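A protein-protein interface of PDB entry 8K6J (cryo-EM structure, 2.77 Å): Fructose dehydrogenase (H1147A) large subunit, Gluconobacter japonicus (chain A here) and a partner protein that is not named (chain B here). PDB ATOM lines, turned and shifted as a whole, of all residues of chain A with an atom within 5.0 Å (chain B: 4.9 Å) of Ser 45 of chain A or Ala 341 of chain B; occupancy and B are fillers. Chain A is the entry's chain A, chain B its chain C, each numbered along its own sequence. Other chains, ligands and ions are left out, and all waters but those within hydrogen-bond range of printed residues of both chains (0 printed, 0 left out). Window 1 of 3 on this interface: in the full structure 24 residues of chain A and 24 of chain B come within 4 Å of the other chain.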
ATOM      1  N   ASP A  43      -7.483  21.839  24.225  1.00  0.00           N
ATOM      2  CA  ASP A  43      -7.403  23.182  24.780  1.00  0.00           C
ATOM      3  C   ASP A  43      -8.261  23.251  26.035  1.00  0.00           C
ATOM      4  O   ASP A  43      -9.418  22.820  26.023  1.00  0.00           O
ATOM      5  CB  ASP A  43      -7.865  24.223  23.761  1.00  0.00           C
ATOM      6  CG  ASP A  43      -6.804  24.528  22.725  1.00  0.00           C
ATOM      7  OD1 ASP A  43      -5.625  24.202  22.968  1.00  0.00           O
ATOM      8  OD2 ASP A  43      -7.147  25.090  21.665  1.00  0.00           O
ATOM      9  N   ARG A  44      -7.692  23.796  27.110  1.00  0.00           N
ATOM     10  CA  ARG A  44      -8.384  23.802  28.394  1.00  0.00           C
ATOM     11  C   ARG A  44      -9.682  24.596  28.325  1.00  0.00           C
ATOM     12  O   ARG A  44     -10.706  24.173  28.873  1.00  0.00           O
ATOM     13  CB  ARG A  44      -7.466  24.366  29.477  1.00  0.00           C
ATOM     14  CG  ARG A  44      -8.194  25.023  30.630  1.00  0.00           C
ATOM     15  CD  ARG A  44      -7.216  25.602  31.625  1.00  0.00           C
ATOM     16  NE  ARG A  44      -6.014  24.788  31.736  1.00  0.00           N
ATOM     17  CZ  ARG A  44      -5.830  23.848  32.651  1.00  0.00           C
ATOM     18  NH1 ARG A  44      -6.754  23.574  33.555  1.00  0.00           N
ATOM     19  NH2 ARG A  44      -4.690  23.166  32.661  1.00  0.00           N
ATOM     20  N   SER A  45      -9.659  25.750  27.660  1.00  0.00           N
ATOM     21  CA  SER A  45     -10.847  26.595  27.607  1.00  0.00           C
ATOM     22  C   SER A  45     -11.979  25.918  26.847  1.00  0.00           C
ATOM     23  O   SER A  45     -13.150  26.047  27.222  1.00  0.00           O
ATOM     24  CB  SER A  45     -10.503  27.939  26.976  1.00  0.00           C
ATOM     25  OG  SER A  45      -9.559  28.632  27.772  1.00  0.00           O
ATOM     26  N   GLN A  46     -11.655  25.198  25.773  1.00  0.00           N
ATOM     27  CA  GLN A  46     -12.693  24.478  25.045  1.00  0.00           C
ATOM     28  C   GLN A  46     -13.290  23.366  25.897  1.00  0.00           C
ATOM     29  O   GLN A  46     -14.498  23.115  25.836  1.00  0.00           O
ATOM     30  CB  GLN A  46     -12.135  23.918  23.742  1.00  0.00           C
ATOM     31  CG  GLN A  46     -13.179  23.242  22.884  1.00  0.00           C
ATOM     32  CD  GLN A  46     -14.425  24.080  22.705  1.00  0.00           C
ATOM     33  OE1 GLN A  46     -14.362  25.215  22.244  1.00  0.00           O
ATOM     34  NE2 GLN A  46     -15.569  23.519  23.067  1.00  0.00           N
ATOM     35  N   ILE A  47     -12.465  22.688  26.693  1.00  0.00           N
ATOM     36  CA  ILE A  47     -12.988  21.673  27.603  1.00  0.00           C
ATOM     37  C   ILE A  47     -13.892  22.312  28.645  1.00  0.00           C
ATOM     38  O   ILE A  47     -14.922  21.746  29.029  1.00  0.00           O
ATOM     39  CB  ILE A  47     -11.836  20.893  28.261  1.00  0.00           C
ATOM     40  CG1 ILE A  47     -10.917  20.291  27.199  1.00  0.00           C
ATOM     41  CG2 ILE A  47     -12.384  19.815  29.170  1.00  0.00           C
ATOM     42  CD1 ILE A  47     -11.642  19.545  26.112  1.00  0.00           C
ATOM     43  N   VAL A  48     -13.520  23.500  29.121  1.00  0.00           N
ATOM     44  CA  VAL A  48     -14.359  24.218  30.078  1.00  0.00           C
ATOM     45  C   VAL A  48     -15.709  24.543  29.453  1.00  0.00           C
ATOM     46  O   VAL A  48     -16.763  24.367  30.074  1.00  0.00           O
ATOM     47  CB  VAL A  48     -13.644  25.489  30.564  1.00  0.00           C
ATOM     48  CG1 VAL A  48     -14.607  26.386  31.302  1.00  0.00           C
ATOM     49  CG2 VAL A  48     -12.478  25.123  31.446  1.00  0.00           C
ATOM     50  N   GLU A  49     -15.692  25.023  28.209  1.00  0.00           N
ATOM     51  CA  GLU A  49     -16.937  25.335  27.518  1.00  0.00           C
ATOM     52  C   GLU A  49     -17.779  24.084  27.307  1.00  0.00           C
ATOM     53  O   GLU A  49     -19.008  24.124  27.438  1.00  0.00           O
ATOM     54  CB  GLU A  49     -16.638  26.015  26.184  1.00  0.00           C
ATOM     55  CG  GLU A  49     -17.871  26.378  25.382  1.00  0.00           C
ATOM     56  CD  GLU A  49     -17.529  26.882  23.996  1.00  0.00           C
ATOM     57  OE1 GLU A  49     -16.950  26.107  23.207  1.00  0.00           O
ATOM     58  OE2 GLU A  49     -17.840  28.052  23.695  1.00  0.00           O
ATOM     59  N   ARG A  52     -19.403  23.274  30.594  1.00  0.00           N
ATOM     60  CA  ARG A  52     -20.475  24.210  30.912  1.00  0.00           C
ATOM     61  C   ARG A  52     -21.749  23.858  30.161  1.00  0.00           C
ATOM     62  O   ARG A  52     -22.853  23.966  30.707  1.00  0.00           O
ATOM     63  CB  ARG A  52     -20.039  25.636  30.584  1.00  0.00           C
ATOM     64  CG  ARG A  52     -19.101  26.259  31.596  1.00  0.00           C
ATOM     65  CD  ARG A  52     -18.269  27.344  30.941  1.00  0.00           C
ATOM     66  NE  ARG A  52     -17.708  28.276  31.909  1.00  0.00           N
ATOM     67  CZ  ARG A  52     -16.767  29.167  31.631  1.00  0.00           C
ATOM     68  NH1 ARG A  52     -16.263  29.281  30.414  1.00  0.00           N
ATOM     69  NH2 ARG A  52     -16.317  29.959  32.597  1.00  0.00           N
ATOM     70  N   LEU B 329     -10.148  24.592  20.566  1.00  0.00           N
ATOM     71  CA  LEU B 329     -11.113  25.572  20.066  1.00  0.00           C
ATOM     72  C   LEU B 329     -10.468  26.399  18.955  1.00  0.00           C
ATOM     73  O   LEU B 329      -9.752  27.379  19.174  1.00  0.00           O
ATOM     74  CB  LEU B 329     -11.638  26.451  21.202  1.00  0.00           C
ATOM     75  CG  LEU B 329     -10.863  27.580  21.905  1.00  0.00           C
ATOM     76  CD1 LEU B 329     -11.665  28.143  23.063  1.00  0.00           C
ATOM     77  CD2 LEU B 329      -9.491  27.142  22.383  1.00  0.00           C
ATOM     78  N   ALA B 337     -17.847  34.316  23.041  1.00  0.00           N
ATOM     79  CA  ALA B 337     -17.629  32.929  23.436  1.00  0.00           C
ATOM     80  C   ALA B 337     -16.195  32.705  23.890  1.00  0.00           C
ATOM     81  O   ALA B 337     -15.951  31.988  24.866  1.00  0.00           O
ATOM     82  CB  ALA B 337     -17.979  31.994  22.281  1.00  0.00           C
ATOM     83  N   LEU B 338     -15.230  33.303  23.188  1.00  0.00           N
ATOM     84  CA  LEU B 338     -13.835  33.174  23.592  1.00  0.00           C
ATOM     85  C   LEU B 338     -13.603  33.783  24.967  1.00  0.00           C
ATOM     86  O   LEU B 338     -12.923  33.187  25.811  1.00  0.00           O
ATOM     87  CB  LEU B 338     -12.927  33.834  22.558  1.00  0.00           C
ATOM     88  CG  LEU B 338     -12.436  32.953  21.413  1.00  0.00           C
ATOM     89  CD1 LEU B 338     -11.804  33.803  20.332  1.00  0.00           C
ATOM     90  CD2 LEU B 338     -11.455  31.919  21.923  1.00  0.00           C
ATOM     91  N   TYR B 339     -14.164  34.969  25.214  1.00  0.00           N
ATOM     92  CA  TYR B 339     -14.013  35.588  26.524  1.00  0.00           C
ATOM     93  C   TYR B 339     -14.640  34.730  27.610  1.00  0.00           C
ATOM     94  O   TYR B 339     -14.068  34.570  28.693  1.00  0.00           O
ATOM     95  CB  TYR B 339     -14.634  36.983  26.528  1.00  0.00           C
ATOM     96  CG  TYR B 339     -14.749  37.583  27.909  1.00  0.00           C
ATOM     97  CD1 TYR B 339     -13.669  38.217  28.501  1.00  0.00           C
ATOM     98  CD2 TYR B 339     -15.935  37.514  28.624  1.00  0.00           C
ATOM     99  CE1 TYR B 339     -13.766  38.763  29.760  1.00  0.00           C
ATOM    100  CE2 TYR B 339     -16.039  38.056  29.884  1.00  0.00           C
ATOM    101  CZ  TYR B 339     -14.953  38.678  30.447  1.00  0.00           C
ATOM    102  OH  TYR B 339     -15.054  39.221  31.703  1.00  0.00           O
ATOM    103  N   GLU B 340     -15.821  34.172  27.343  1.00  0.00           N
ATOM    104  CA  GLU B 340     -16.474  33.340  28.344  1.00  0.00           C
ATOM    105  C   GLU B 340     -15.666  32.083  28.632  1.00  0.00           C
ATOM    106  O   GLU B 340     -15.549  31.662  29.788  1.00  0.00           O
ATOM    107  CB  GLU B 340     -17.884  32.975  27.895  1.00  0.00           C
ATOM    108  CG  GLU B 340     -18.697  32.305  28.978  1.00  0.00           C
ATOM    109  CD  GLU B 340     -19.341  33.300  29.917  1.00  0.00           C
ATOM    110  OE1 GLU B 340     -19.153  34.518  29.715  1.00  0.00           O
ATOM    111  OE2 GLU B 340     -20.041  32.868  30.854  1.00  0.00           O
ATOM    112  N   ALA B 341     -15.103  31.468  27.593  1.00  0.00           N
ATOM    113  CA  ALA B 341     -14.352  30.236  27.794  1.00  0.00           C
ATOM    114  C   ALA B 341     -13.043  30.496  28.526  1.00  0.00           C
ATOM    115  O   ALA B 341     -12.657  29.721  29.409  1.00  0.00           O
ATOM    116  CB  ALA B 341     -14.091  29.557  26.453  1.00  0.00           C
ATOM    117  N   VAL B 342     -12.349  31.576  28.187  1.00  0.00           N
ATOM    118  CA  VAL B 342     -10.996  31.813  28.675  1.00  0.00           C
ATOM    119  C   VAL B 342     -10.983  32.689  29.920  1.00  0.00           C
ATOM    120  O   VAL B 342     -10.322  32.366  30.906  1.00  0.00           O
ATOM    121  CB  VAL B 342     -10.123  32.422  27.558  1.00  0.00           C
ATOM    122  CG1 VAL B 342      -8.694  32.564  28.030  1.00  0.00           C
ATOM    123  CG2 VAL B 342     -10.188  31.564  26.312  1.00  0.00           C
ATOM    124  N   CYS B 343     -11.712  33.806  29.899  1.00  0.00           N
ATOM    125  CA  CYS B 343     -11.555  34.829  30.922  1.00  0.00           C
ATOM    126  C   CYS B 343     -12.718  34.940  31.895  1.00  0.00           C
ATOM    127  O   CYS B 343     -12.533  35.501  32.978  1.00  0.00           O
ATOM    128  CB  CYS B 343     -11.336  36.200  30.267  1.00  0.00           C
ATOM    129  SG  CYS B 343     -10.730  36.126  28.571  1.00  0.00           S
ATOM    130  N   GLN B 405      -3.656  28.355  28.914  1.00  0.00           N
ATOM    131  CA  GLN B 405      -4.362  28.319  27.633  1.00  0.00           C
ATOM    132  C   GLN B 405      -3.633  29.220  26.652  1.00  0.00           C
ATOM    133  O   GLN B 405      -3.800  30.448  26.678  1.00  0.00           O
ATOM    134  CB  GLN B 405      -5.819  28.746  27.785  1.00  0.00           C
ATOM    135  CG  GLN B 405      -6.574  28.839  26.475  1.00  0.00           C
ATOM    136  CD  GLN B 405      -6.373  27.623  25.604  1.00  0.00           C
ATOM    137  OE1 GLN B 405      -6.873  26.542  25.904  1.00  0.00           O
ATOM    138  NE2 GLN B 405      -5.636  27.791  24.515  1.00  0.00           N
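The side-chain carboxylate (OD2) of Asp 43 of chain A sits close to the backbone NH (N) of Leu 329 of chain B (3.2 Å).
N of Arg 44 of chain A sits at hydrogen-bond distance from OE1 of Gln 405 of chain B (3.1 Å).
The side-chain amide oxygen (OE1) of Gln 405 of chain B sits at hydrogen-bond distance from the backbone NH (N) of Ser 45 of chain A.
NH1 of Arg 52 of chain A lies within hydrogen-bond range of O of Glu 340 of chain B (2.6 Å).
Printed residues of chain B within 4 Å of Asp 43 of chain A: Leu 329 and Gln 405.
Ile 47 of chain A touches none of the printed residues of chain B.
Of the printed residues of chain B, Arg 52 of chain A touches Glu 340 and Ala 341.
Printed residues of chain A within 4 Å of Glu 340 of chain B: Arg 52.
Ala 341 of chain B touches just these residues of chain A: Ser 45 and Arg 52.
Of the printed residues of chain A, Val 342 of chain B touches Ser 45 (3.3 Å).
Cys 343 of chain B touches none of the printed residues of chain A.
The nearest residue of chain B that does not touch Ser 45 of chain A is Leu 329 of chain B (4.1 Å).
The nearest residue of chain A that does not touch Ala 341 of chain B is Val 48 of chain A (4.3 Å).
Of the 9 printed residues of chain B, 5 touch a printed residue of chain A.
Of the 8 printed residues of chain A, 5 touch a printed residue of chain B.
Among the printed residues, no Asp or Glu carboxylate lies within 4 Å of a Lys or Arg side-chain nitrogen of the other chain.
The side-chain carboxylate (OE1) of Glu 49 of chain A lies close to the side-chain amide oxygen (OE1) of Gln 46 of chain A, 2.9 Å away.
Among the printed residues, merely in contact across the chains: Gln 46 of chain A with Leu 329 of chain B, Asp 43 of chain A with Gln 405 of chain B, Ser 45 of chain A with Val 342 of chain B, Arg 52 of chain A with Ala 341 of chain B and Ser 45 of chain A with Ala 341 of chain B.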
